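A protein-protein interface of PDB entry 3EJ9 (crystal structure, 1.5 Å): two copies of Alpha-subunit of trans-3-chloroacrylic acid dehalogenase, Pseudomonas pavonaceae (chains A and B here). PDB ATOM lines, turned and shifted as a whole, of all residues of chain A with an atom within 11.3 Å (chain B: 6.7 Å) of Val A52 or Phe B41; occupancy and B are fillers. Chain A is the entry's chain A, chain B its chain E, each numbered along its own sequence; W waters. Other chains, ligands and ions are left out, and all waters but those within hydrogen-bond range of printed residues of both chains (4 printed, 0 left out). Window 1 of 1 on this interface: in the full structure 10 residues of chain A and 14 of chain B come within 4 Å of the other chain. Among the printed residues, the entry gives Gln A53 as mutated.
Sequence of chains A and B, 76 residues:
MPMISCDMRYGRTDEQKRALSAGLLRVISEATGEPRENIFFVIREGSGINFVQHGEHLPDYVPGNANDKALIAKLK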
ATOM      1  N   ASP A   7      12.699  27.495   5.678  1.00  0.00           N
ATOM      2  CA  ASP A   7      12.290  27.025   7.003  1.00  0.00           C
ATOM      3  C   ASP A   7      12.767  25.592   7.166  1.00  0.00           C
ATOM      4  O   ASP A   7      12.419  24.726   6.371  1.00  0.00           O
ATOM      5  CB  ASP A   7      10.768  27.071   7.167  1.00  0.00           C
ATOM      6  CG  ASP A   7      10.235  28.472   7.405  1.00  0.00           C
ATOM      7  OD1 ASP A   7       9.959  28.800   8.574  1.00  0.00           O
ATOM      8  OD2 ASP A   7      10.078  29.235   6.428  1.00  0.00           O
ATOM      9  N   MET A   8      13.550  25.332   8.207  1.00  0.00           N
ATOM     10  CA  MET A   8      14.038  23.974   8.459  1.00  0.00           C
ATOM     11  C   MET A   8      14.276  23.753   9.943  1.00  0.00           C
ATOM     12  O   MET A   8      14.342  24.699  10.725  1.00  0.00           O
ATOM     13  CB  MET A   8      15.310  23.685   7.663  1.00  0.00           C
ATOM     14  CG  MET A   8      16.536  24.465   8.100  1.00  0.00           C
ATOM     15  SD  MET A   8      17.900  23.937   7.049  1.00  0.00           S
ATOM     16  CE  MET A   8      19.197  25.014   7.642  1.00  0.00           C
ATOM     17  N   ARG A   9      14.412  22.490  10.324  1.00  0.00           N
ATOM     18  CA  ARG A   9      14.671  22.159  11.712  1.00  0.00           C
ATOM     19  C   ARG A   9      16.006  22.712  12.188  1.00  0.00           C
ATOM     20  O   ARG A   9      17.005  22.719  11.463  1.00  0.00           O
ATOM     21  CB  ARG A   9      14.640  20.643  11.915  1.00  0.00           C
ATOM     22  CG  ARG A   9      13.249  20.048  11.819  1.00  0.00           C
ATOM     23  CD  ARG A   9      13.336  18.531  11.893  1.00  0.00           C
ATOM     24  NE  ARG A   9      13.940  18.020  10.671  1.00  0.00           N
ATOM     25  CZ  ARG A   9      14.406  16.793  10.498  1.00  0.00           C
ATOM     26  NH1 ARG A   9      14.332  15.891  11.475  1.00  0.00           N
ATOM     27  NH2 ARG A   9      14.934  16.461   9.327  1.00  0.00           N
ATOM     28  N   ARG A  44      15.115  30.126   8.565  1.00  0.00           N
ATOM     29  CA  ARG A  44      14.294  30.165   9.772  1.00  0.00           C
ATOM     30  C   ARG A  44      14.289  28.773  10.375  1.00  0.00           C
ATOM     31  O   ARG A  44      14.002  27.798   9.690  1.00  0.00           O
ATOM     32  CB  ARG A  44      12.864  30.573   9.438  1.00  0.00           C
ATOM     33  CG  ARG A  44      12.739  31.910   8.761  1.00  0.00           C
ATOM     34  CD  ARG A  44      11.276  32.253   8.617  1.00  0.00           C
ATOM     35  NE  ARG A  44      11.124  33.460   7.813  1.00  0.00           N
ATOM     36  CZ  ARG A  44      10.565  33.512   6.608  1.00  0.00           C
ATOM     37  NH1 ARG A  44      10.091  32.410   6.038  1.00  0.00           N
ATOM     38  NH2 ARG A  44      10.468  34.671   5.979  1.00  0.00           N
ATOM     39  N   GLY A  46      13.384  25.919  13.636  1.00  0.00           N
ATOM     40  CA  GLY A  46      12.524  25.583  14.763  1.00  0.00           C
ATOM     41  C   GLY A  46      12.677  24.140  15.193  1.00  0.00           C
ATOM     42  O   GLY A  46      13.402  23.360  14.562  1.00  0.00           O
ATOM     43  N   SER A  47      11.997  23.785  16.281  1.00  0.00           N
ATOM     44  CA  SER A  47      11.974  22.415  16.791  1.00  0.00           C
ATOM     45  C   SER A  47      11.312  21.445  15.811  1.00  0.00           C
ATOM     46  O   SER A  47      10.466  21.850  15.027  1.00  0.00           O
ATOM     47  CB  SER A  47      11.233  22.394  18.126  1.00  0.00           C
ATOM     48  OG  SER A  47      11.816  23.313  19.048  1.00  0.00           O
ATOM     49  N   GLY A  48      11.705  20.174  15.853  1.00  0.00           N
ATOM     50  CA  GLY A  48      11.141  19.160  14.956  1.00  0.00           C
ATOM     51  C   GLY A  48       9.626  19.042  14.965  1.00  0.00           C
ATOM     52  O   GLY A  48       8.986  18.913  13.917  1.00  0.00           O
ATOM     53  N   ILE A  49       9.051  19.115  16.159  1.00  0.00           N
ATOM     54  CA  ILE A  49       7.602  19.035  16.348  1.00  0.00           C
ATOM     55  C   ILE A  49       6.874  20.130  15.558  1.00  0.00           C
ATOM     56  O   ILE A  49       5.695  19.995  15.247  1.00  0.00           O
ATOM     57  CB  ILE A  49       7.236  19.088  17.865  1.00  0.00           C
ATOM     58  CG1 ILE A  49       5.758  18.764  18.113  1.00  0.00           C
ATOM     59  CG2 ILE A  49       7.596  20.445  18.476  1.00  0.00           C
ATOM     60  CD1 ILE A  49       5.448  17.304  18.279  1.00  0.00           C
ATOM     61  N   ASN A  50       7.594  21.192  15.204  1.00  0.00           N
ATOM     62  CA  ASN A  50       7.003  22.285  14.457  1.00  0.00           C
ATOM     63  C   ASN A  50       6.866  22.010  12.958  1.00  0.00           C
ATOM     64  O   ASN A  50       6.280  22.825  12.242  1.00  0.00           O
ATOM     65  CB  ASN A  50       7.839  23.551  14.665  1.00  0.00           C
ATOM     66  CG  ASN A  50       7.669  24.156  16.045  1.00  0.00           C
ATOM     67  OD1 ASN A  50       6.906  23.658  16.877  1.00  0.00           O
ATOM     68  ND2 ASN A  50       8.379  25.243  16.292  1.00  0.00           N
ATOM     69  N   PHE A  51       7.404  20.872  12.505  1.00  0.00           N
ATOM     70  CA  PHE A  51       7.414  20.531  11.077  1.00  0.00           C
ATOM     71  C   PHE A  51       6.575  19.302  10.840  1.00  0.00           C
ATOM     72  O   PHE A  51       6.772  18.269  11.490  1.00  0.00           O
ATOM     73  CB  PHE A  51       8.842  20.320  10.570  1.00  0.00           C
ATOM     74  CG  PHE A  51       9.644  21.586  10.522  1.00  0.00           C
ATOM     75  CD1 PHE A  51      10.198  22.121  11.694  1.00  0.00           C
ATOM     76  CD2 PHE A  51       9.831  22.270   9.320  1.00  0.00           C
ATOM     77  CE1 PHE A  51      10.910  23.308  11.667  1.00  0.00           C
ATOM     78  CE2 PHE A  51      10.550  23.456   9.292  1.00  0.00           C
ATOM     79  CZ  PHE A  51      11.087  23.979  10.464  1.00  0.00           C
ATOM     80  N   VAL A  52       5.630  19.435   9.916  1.00  0.00           N
ATOM     81  CA  VAL A  52       4.667  18.374   9.666  1.00  0.00           C
ATOM     82  C   VAL A  52       4.660  18.035   8.181  1.00  0.00           C
ATOM     83  O   VAL A  52       4.286  18.859   7.344  1.00  0.00           O
ATOM     84  CB  VAL A  52       3.247  18.742  10.179  1.00  0.00           C
ATOM     85  CG1 VAL A  52       2.357  17.533  10.162  1.00  0.00           C
ATOM     86  CG2 VAL A  52       3.313  19.281  11.596  1.00  0.00           C
ATOM     87  N   GLN A  53       5.099  16.820   7.853  1.00  0.00           N
ATOM     88  CA  GLN A  53       5.119  16.366   6.466  1.00  0.00           C
ATOM     89  C   GLN A  53       4.186  15.176   6.389  1.00  0.00           C
ATOM     90  O   GLN A  53       4.300  14.248   7.192  1.00  0.00           O
ATOM     91  CB  GLN A  53       6.533  15.958   6.050  1.00  0.00           C
ATOM     92  CG  GLN A  53       6.705  15.732   4.547  1.00  0.00           C
ATOM     93  CD  GLN A  53       6.950  17.023   3.804  1.00  0.00           C
ATOM     94  OE1 GLN A  53       7.857  17.779   4.145  1.00  0.00           O
ATOM     95  NE2 GLN A  53       6.134  17.291   2.785  1.00  0.00           N
ATOM     96  N   HIS A  54       3.270  15.216   5.419  1.00  0.00           N
ATOM     97  CA  HIS A  54       2.146  14.275   5.295  1.00  0.00           C
ATOM     98  C   HIS A  54       1.453  13.933   6.622  1.00  0.00           C
ATOM     99  O   HIS A  54       1.096  12.784   6.881  1.00  0.00           O
ATOM    100  CB  HIS A  54       2.535  13.017   4.505  1.00  0.00           C
ATOM    101  CG  HIS A  54       3.630  12.211   5.129  1.00  0.00           C
ATOM    102  ND1 HIS A  54       4.946  12.306   4.724  1.00  0.00           N
ATOM    103  CD2 HIS A  54       3.602  11.290   6.126  1.00  0.00           C
ATOM    104  CE1 HIS A  54       5.684  11.485   5.451  1.00  0.00           C
ATOM    105  NE2 HIS A  54       4.892  10.854   6.307  1.00  0.00           N
ATOM    106  N   GLY A  55       1.253  14.950   7.451  1.00  0.00           N
ATOM    107  CA  GLY A  55       0.530  14.774   8.702  1.00  0.00           C
ATOM    108  C   GLY A  55       1.360  14.275   9.863  1.00  0.00           C
ATOM    109  O   GLY A  55       0.880  14.240  11.000  1.00  0.00           O
ATOM    110  N   GLU A  56       2.607  13.898   9.590  1.00  0.00           N
ATOM    111  CA  GLU A  56       3.502  13.404  10.628  1.00  0.00           C
ATOM    112  C   GLU A  56       4.478  14.472  11.070  1.00  0.00           C
ATOM    113  O   GLU A  56       5.149  15.094  10.239  1.00  0.00           O
ATOM    114  CB  GLU A  56       4.266  12.166  10.146  1.00  0.00           C
ATOM    115  CG  GLU A  56       3.461  10.883  10.166  1.00  0.00           C
ATOM    116  CD  GLU A  56       4.146   9.739   9.442  1.00  0.00           C
ATOM    117  OE1 GLU A  56       5.352   9.851   9.116  1.00  0.00           O
ATOM    118  OE2 GLU A  56       3.473   8.722   9.206  1.00  0.00           O
ATOM    119  N   HIS A  57       4.539  14.677  12.382  1.00  0.00           N
ATOM    120  CA  HIS A  57       5.470  15.632  12.985  1.00  0.00           C
ATOM    121  C   HIS A  57       6.884  15.034  12.951  1.00  0.00           C
ATOM    122  O   HIS A  57       7.090  13.859  13.263  1.00  0.00           O
ATOM    123  CB  HIS A  57       5.029  15.954  14.422  1.00  0.00           C
ATOM    124  CG  HIS A  57       3.760  16.753  14.496  1.00  0.00           C
ATOM    125  ND1 HIS A  57       3.733  18.079  14.875  1.00  0.00           N
ATOM    126  CD2 HIS A  57       2.477  16.419  14.212  1.00  0.00           C
ATOM    127  CE1 HIS A  57       2.488  18.522  14.839  1.00  0.00           C
ATOM    128  NE2 HIS A  57       1.708  17.536  14.428  1.00  0.00           N
ATOM    129  N   LEU A  58       7.856  15.844  12.544  1.00  0.00           N
ATOM    130  CA  LEU A  58       9.227  15.374  12.399  1.00  0.00           C
ATOM    131  C   LEU A  58       9.916  15.253  13.754  1.00  0.00           C
ATOM    132  O   LEU A  58       9.555  15.952  14.705  1.00  0.00           O
ATOM    133  CB  LEU A  58      10.023  16.305  11.472  1.00  0.00           C
ATOM    134  CG  LEU A  58       9.548  16.432  10.020  1.00  0.00           C
ATOM    135  CD1 LEU A  58      10.572  17.203   9.194  1.00  0.00           C
ATOM    136  CD2 LEU A  58       9.280  15.079   9.389  1.00  0.00           C
ATOM    137  N   PRO A  59      10.910  14.362  13.848  1.00  0.00           N
ATOM    138  CA  PRO A  59      11.733  14.344  15.050  1.00  0.00           C
ATOM    139  C   PRO A  59      12.726  15.498  14.982  1.00  0.00           C
ATOM    140  O   PRO A  59      12.934  16.073  13.915  1.00  0.00           O
ATOM    141  CB  PRO A  59      12.466  13.007  14.940  1.00  0.00           C
ATOM    142  CG  PRO A  59      12.592  12.781  13.476  1.00  0.00           C
ATOM    143  CD  PRO A  59      11.335  13.351  12.866  1.00  0.00           C
ATOM    144  N   ASP A  60      13.353  15.823  16.106  1.00  0.00           N
ATOM    145  CA  ASP A  60      14.440  16.794  16.081  1.00  0.00           C
ATOM    146  C   ASP A  60      15.555  16.314  15.164  1.00  0.00           C
ATOM    147  O   ASP A  60      15.796  15.104  15.033  1.00  0.00           O
ATOM    148  CB  ASP A  60      14.995  17.031  17.486  1.00  0.00           C
ATOM    149  CG  ASP A  60      14.093  17.908  18.346  1.00  0.00           C
ATOM    150  OD1 ASP A  60      14.304  17.953  19.572  1.00  0.00           O
ATOM    151  OD2 ASP A  60      13.173  18.562  17.814  1.00  0.00           O
ATOM    152  N   PRO B   2      -0.505  21.804  -0.823  1.00  0.00           N
ATOM    153  CA  PRO B   2      -0.641  23.042  -0.076  1.00  0.00           C
ATOM    154  C   PRO B   2       0.437  23.176   0.970  1.00  0.00           C
ATOM    155  O   PRO B   2       0.939  22.174   1.476  1.00  0.00           O
ATOM    156  CB  PRO B   2      -2.002  22.878   0.605  1.00  0.00           C
ATOM    157  CG  PRO B   2      -2.790  22.087  -0.372  1.00  0.00           C
ATOM    158  CD  PRO B   2      -1.823  21.227  -1.154  1.00  0.00           C
ATOM    159  N   MET B   3       0.789  24.420   1.281  1.00  0.00           N
ATOM    160  CA  MET B   3       1.732  24.706   2.357  1.00  0.00           C
ATOM    161  C   MET B   3       1.078  25.684   3.315  1.00  0.00           C
ATOM    162  O   MET B   3       0.531  26.710   2.908  1.00  0.00           O
ATOM    163  CB  MET B   3       3.056  25.281   1.843  1.00  0.00           C
ATOM    164  CG  MET B   3       3.816  24.420   0.855  1.00  0.00           C
ATOM    165  SD  MET B   3       3.448  24.990  -0.805  1.00  0.00           S
ATOM    166  CE  MET B   3       4.610  24.052  -1.777  1.00  0.00           C
ATOM    167  N   ILE B   4       1.142  25.354   4.591  1.00  0.00           N
ATOM    168  CA  ILE B   4       0.503  26.141   5.631  1.00  0.00           C
ATOM    169  C   ILE B   4       1.576  26.522   6.635  1.00  0.00           C
ATOM    170  O   ILE B   4       2.398  25.699   7.002  1.00  0.00           O
ATOM    171  CB  ILE B   4      -0.595  25.317   6.373  1.00  0.00           C
ATOM    172  CG1 ILE B   4      -1.512  24.565   5.401  1.00  0.00           C
ATOM    173  CG2 ILE B   4      -1.393  26.222   7.327  1.00  0.00           C
ATOM    174  CD1 ILE B   4      -2.304  23.479   6.071  1.00  0.00           C
ATOM    175  N   SER B   5       1.557  27.776   7.080  1.00  0.00           N
ATOM    176  CA  SER B   5       2.395  28.168   8.215  1.00  0.00           C
ATOM    177  C   SER B   5       1.572  28.803   9.320  1.00  0.00           C
ATOM    178  O   SER B   5       0.522  29.392   9.074  1.00  0.00           O
ATOM    179  CB  SER B   5       3.512  29.108   7.789  1.00  0.00           C
ATOM    180  OG  SER B   5       2.995  30.306   7.249  1.00  0.00           O
ATOM    181  N   CYS B   6       2.056  28.672  10.547  1.00  0.00           N
ATOM    182  CA  CYS B   6       1.411  29.294  11.691  1.00  0.00           C
ATOM    183  C   CYS B   6       2.469  29.937  12.565  1.00  0.00           C
ATOM    184  O   CYS B   6       3.280  29.228  13.163  1.00  0.00           O
ATOM    185  CB  CYS B   6       0.629  28.259  12.502  1.00  0.00           C
ATOM    186  SG  CYS B   6      -0.117  28.911  14.009  1.00  0.00           S
ATOM    187  N   LYS B  17       0.009  21.246  19.578  1.00  0.00           N
ATOM    188  CA  LYS B  17       0.565  21.373  18.231  1.00  0.00           C
ATOM    189  C   LYS B  17       0.055  20.262  17.326  1.00  0.00           C
ATOM    190  O   LYS B  17      -0.258  20.500  16.153  1.00  0.00           O
ATOM    191  CB  LYS B  17       2.086  21.364  18.275  1.00  0.00           C
ATOM    192  CG  LYS B  17       2.664  22.598  18.933  1.00  0.00           C
ATOM    193  CD  LYS B  17       4.173  22.564  18.944  1.00  0.00           C
ATOM    194  CE  LYS B  17       4.721  23.863  19.493  1.00  0.00           C
ATOM    195  NZ  LYS B  17       6.200  23.807  19.595  1.00  0.00           N
ATOM    196  N   LEU B  20      -3.560  21.026  16.442  1.00  0.00           N
ATOM    197  CA  LEU B  20      -3.584  22.104  15.477  1.00  0.00           C
ATOM    198  C   LEU B  20      -3.298  21.571  14.082  1.00  0.00           C
ATOM    199  O   LEU B  20      -4.037  21.867  13.152  1.00  0.00           O
ATOM    200  CB  LEU B  20      -2.580  23.195  15.869  1.00  0.00           C
ATOM    201  CG  LEU B  20      -2.511  24.407  14.944  1.00  0.00           C
ATOM    202  CD1 LEU B  20      -3.846  25.144  14.925  1.00  0.00           C
ATOM    203  CD2 LEU B  20      -1.390  25.321  15.404  1.00  0.00           C
ATOM    204  N   SER B  21      -2.231  20.787  13.932  1.00  0.00           N
ATOM    205  CA  SER B  21      -1.868  20.272  12.611  1.00  0.00           C
ATOM    206  C   SER B  21      -2.976  19.364  12.071  1.00  0.00           C
ATOM    207  O   SER B  21      -3.368  19.485  10.917  1.00  0.00           O
ATOM    208  CB  SER B  21      -0.524  19.536  12.642  1.00  0.00           C
ATOM    209  OG  SER B  21      -0.656  18.229  13.147  1.00  0.00           O
ATOM    210  N   ALA B  22      -3.512  18.480  12.909  1.00  0.00           N
ATOM    211  CA  ALA B  22      -4.563  17.586  12.459  1.00  0.00           C
ATOM    212  C   ALA B  22      -5.772  18.368  11.955  1.00  0.00           C
ATOM    213  O   ALA B  22      -6.334  18.019  10.914  1.00  0.00           O
ATOM    214  CB  ALA B  22      -4.960  16.624  13.569  1.00  0.00           C
ATOM    215  N   LEU B  24      -5.992  21.659  10.964  1.00  0.00           N
ATOM    216  CA  LEU B  24      -5.684  22.443   9.756  1.00  0.00           C
ATOM    217  C   LEU B  24      -5.574  21.566   8.512  1.00  0.00           C
ATOM    218  O   LEU B  24      -6.083  21.922   7.450  1.00  0.00           O
ATOM    219  CB  LEU B  24      -4.420  23.296   9.933  1.00  0.00           C
ATOM    220  CG  LEU B  24      -4.523  24.433  10.956  1.00  0.00           C
ATOM    221  CD1 LEU B  24      -3.159  25.053  11.190  1.00  0.00           C
ATOM    222  CD2 LEU B  24      -5.539  25.497  10.530  1.00  0.00           C
ATOM    223  N   LEU B  25      -4.918  20.419   8.645  1.00  0.00           N
ATOM    224  CA  LEU B  25      -4.829  19.474   7.536  1.00  0.00           C
ATOM    225  C   LEU B  25      -6.204  19.014   7.065  1.00  0.00           C
ATOM    226  O   LEU B  25      -6.466  18.976   5.871  1.00  0.00           O
ATOM    227  CB  LEU B  25      -3.948  18.280   7.905  1.00  0.00           C
ATOM    228  CG  LEU B  25      -2.473  18.346   7.493  1.00  0.00           C
ATOM    229  CD1 LEU B  25      -1.763  19.611   7.978  1.00  0.00           C
ATOM    230  CD2 LEU B  25      -1.767  17.133   8.027  1.00  0.00           C
ATOM    231  N   ILE B  39       0.229  17.847   1.698  1.00  0.00           N
ATOM    232  CA  ILE B  39       0.132  19.026   2.555  1.00  0.00           C
ATOM    233  C   ILE B  39       1.365  19.122   3.449  1.00  0.00           C
ATOM    234  O   ILE B  39       1.800  18.125   4.019  1.00  0.00           O
ATOM    235  CB  ILE B  39      -1.183  19.008   3.403  1.00  0.00           C
ATOM    236  CG1 ILE B  39      -2.418  18.956   2.497  1.00  0.00           C
ATOM    237  CG2 ILE B  39      -1.275  20.215   4.334  1.00  0.00           C
ATOM    238  CD1 ILE B  39      -3.714  18.605   3.223  1.00  0.00           C
ATOM    239  N   PHE B  40       1.937  20.327   3.534  1.00  0.00           N
ATOM    240  CA  PHE B  40       3.051  20.622   4.432  1.00  0.00           C
ATOM    241  C   PHE B  40       2.616  21.711   5.414  1.00  0.00           C
ATOM    242  O   PHE B  40       1.947  22.666   5.015  1.00  0.00           O
ATOM    243  CB  PHE B  40       4.289  21.085   3.641  1.00  0.00           C
ATOM    244  CG  PHE B  40       5.368  21.638   4.510  1.00  0.00           C
ATOM    245  CD1 PHE B  40       6.235  20.782   5.188  1.00  0.00           C
ATOM    246  CD2 PHE B  40       5.495  23.017   4.692  1.00  0.00           C
ATOM    247  CE1 PHE B  40       7.229  21.287   6.019  1.00  0.00           C
ATOM    248  CE2 PHE B  40       6.487  23.525   5.523  1.00  0.00           C
ATOM    249  CZ  PHE B  40       7.350  22.662   6.186  1.00  0.00           C
ATOM    250  N   PHE B  41       3.033  21.589   6.671  1.00  0.00           N
ATOM    251  CA  PHE B  41       2.709  22.569   7.714  1.00  0.00           C
ATOM    252  C   PHE B  41       3.929  22.863   8.586  1.00  0.00           C
ATOM    253  O   PHE B  41       4.654  21.951   8.995  1.00  0.00           O
ATOM    254  CB  PHE B  41       1.541  22.022   8.557  1.00  0.00           C
ATOM    255  CG  PHE B  41       1.154  22.882   9.748  1.00  0.00           C
ATOM    256  CD1 PHE B  41       0.861  24.235   9.609  1.00  0.00           C
ATOM    257  CD2 PHE B  41       1.052  22.312  11.006  1.00  0.00           C
ATOM    258  CE1 PHE B  41       0.491  25.009  10.723  1.00  0.00           C
ATOM    259  CE2 PHE B  41       0.674  23.065  12.113  1.00  0.00           C
ATOM    260  CZ  PHE B  41       0.385  24.408  11.975  1.00  0.00           C
ATOM    261  N   VAL B  42       4.131  24.157   8.852  1.00  0.00           N
ATOM    262  CA  VAL B  42       5.203  24.593   9.752  1.00  0.00           C
ATOM    263  C   VAL B  42       4.676  25.614  10.770  1.00  0.00           C
ATOM    264  O   VAL B  42       3.966  26.555  10.426  1.00  0.00           O
ATOM    265  CB  VAL B  42       6.450  25.135   8.974  1.00  0.00           C
ATOM    266  CG1 VAL B  42       6.102  26.342   8.104  1.00  0.00           C
ATOM    267  CG2 VAL B  42       7.580  25.484   9.937  1.00  0.00           C
ATOM    268  N   ILE B  43       5.032  25.383  12.033  1.00  0.00           N
ATOM    269  CA  ILE B  43       4.779  26.302  13.135  1.00  0.00           C
ATOM    270  C   ILE B  43       6.066  27.095  13.363  1.00  0.00           C
ATOM    271  O   ILE B  43       7.142  26.512  13.447  1.00  0.00           O
ATOM    272  CB  ILE B  43       4.417  25.526  14.411  1.00  0.00           C
ATOM    273  CG1 ILE B  43       3.068  24.824  14.243  1.00  0.00           C
ATOM    274  CG2 ILE B  43       4.394  26.452  15.622  1.00  0.00           C
ATOM    275  CD1 ILE B  43       2.793  23.779  15.310  1.00  0.00           C
HETATM  276  O   HOH W   1      -1.247  15.976  11.610  1.00  0.00           O
HETATM  277  O   HOH W   2       3.484  16.283   2.859  1.00  0.00           O
HETATM  278  O   HOH W   3      -1.194  15.673  14.492  1.00  0.00           O
HETATM  279  O   HOH W   4       1.555  17.840   6.846  1.00  0.00           O
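OD1 of Asn A50 is in hydrogen-bond range of NZ of Lys B17, at 2.8 Å.
O of Asn A50 is in hydrogen-bond range of N of Ile B43 (2.9 Å).
The backbone NH of Val A52 lies within hydrogen-bond range of the backbone carbonyl oxygen of Phe B41 (2.9 Å).
The side-chain hydroxyl (OG) of Ser B21 sits at hydrogen-bond distance from a ring nitrogen (NE2) of His A57.
Printed residues of chain B within 4 Å of Val A52: Ser B21 (3.99 Å), Phe B40 (3.5 Å) and Phe B41 (2.9 Å).
Of the printed residues of chain B, His A57 touches Lys B17 and Ser B21.
No residue of chain A comes within 4 Å of Ile B4.
Ser B5 touches none of the printed residues of chain A.
No residue of chain A comes within 4 Å of Cys B6.
Of the printed residues of chain A, Lys B17 touches Ile A49 (3.8 Å), Asn A50 (2.8 Å) and His A57 (3.6 Å).
Of chain A, only Asn A50 (3.7 Å), Phe A51 (3.7 Å) and Val A52 (2.9 Å) come within 4 Å of Phe B41.
Printed residues of chain A within 4 Å of Val B42: Asn A50 and Phe A51.
Ile B43 touches one residue of chain A.
The nearest printed residue of chain B that does not touch Val A52 is Ile B39 (4.2 Å).
ND1 of His A57 lies within hydrogen-bond range of O of Ile A49 (2.8 Å).
The backbone NH (N) of Leu A58 lies within hydrogen-bond range of the backbone carbonyl oxygen (O) of Phe A51 (2.9 Å).
The side-chain carboxylate of Glu A56 is in hydrogen-bond range of a ring nitrogen (NE2) of His A54 (3.0 Å).
The backbone carbonyl oxygen (O) of Pro B2 sits at hydrogen-bond distance from the backbone NH (N) of Phe B40, 2.9 Å away.
The backbone NH (N) of Ile B4 lies within hydrogen-bond range of the backbone carbonyl oxygen (O) of Phe B40 (2.8 Å).
O of Ile B4 is in hydrogen-bond range of N of Val B42 (3.0 Å).
No position is printed for both chains.
Of the 15 pairs that touch across the chains among the printed residues, none has its exchanged pair printed and touching as well.
Water W2 lies within hydrogen-bond range of the backbone carbonyl oxygen (O) of Ile B39, the backbone NH (N) of His A54 and the side-chain amide nitrogen (NE2) of Gln A53.
Water W1 bridges OG of Ser B21 (2.8 Å) and O of Gly A55 (2.8 Å).
Water W4 lies within hydrogen-bond range of the backbone carbonyl oxygen (O) of Ile B39 (2.9 Å), the backbone carbonyl oxygen (O) of Val A52 (3.0 Å), the backbone NH (N) of Gly A55 (3.0 Å) and the backbone NH (N) of His A54 (3.4 Å).
Water W3 lies within hydrogen-bond range of OG of Ser B21 (2.9 Å) and NE2 of His A57 (3.4 Å).
NZ of Lys B17 touches CG2 of Ile A49, at 3.8 Å.
Asn A50 touches Phe B41 (O to O, 3.7 Å).
O of Asn A50 touches CA of Val B42, at 3.2 Å.
Phe A51 touches Phe B41.
CE2 of Phe A51 touches CG2 of Val B42 (3.7 Å).
CG2 of Val A52 touches CB of Ser B21, at 3.99 Å.
Val A52 touches Phe B40 (O to CD1, 3.5 Å).
Phe B40 touches Gln A53.
Leu B25 touches Gly A55 (CD2 to CA, 3.4 Å).
Lys B17 touches His A57 (O to CE1, 3.6 Å).
Of the 19 printed residues of chain A, 8 touch a printed residue of chain B.
Of the 16 printed residues of chain B, 8 touch a printed residue of chain A.
Printed residues of chain B that touch a printed residue of chain A: Lys B17, Ser B21, Leu B25, Ile B39, Phe B40, Phe B41, Val B42 and Ile B43.
Hydrophobic or aromatic side chains of chain B within 4 Å of the printed part of chain A: Leu B25, Phe B40, Phe B41, Val B42 and Ile B43.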
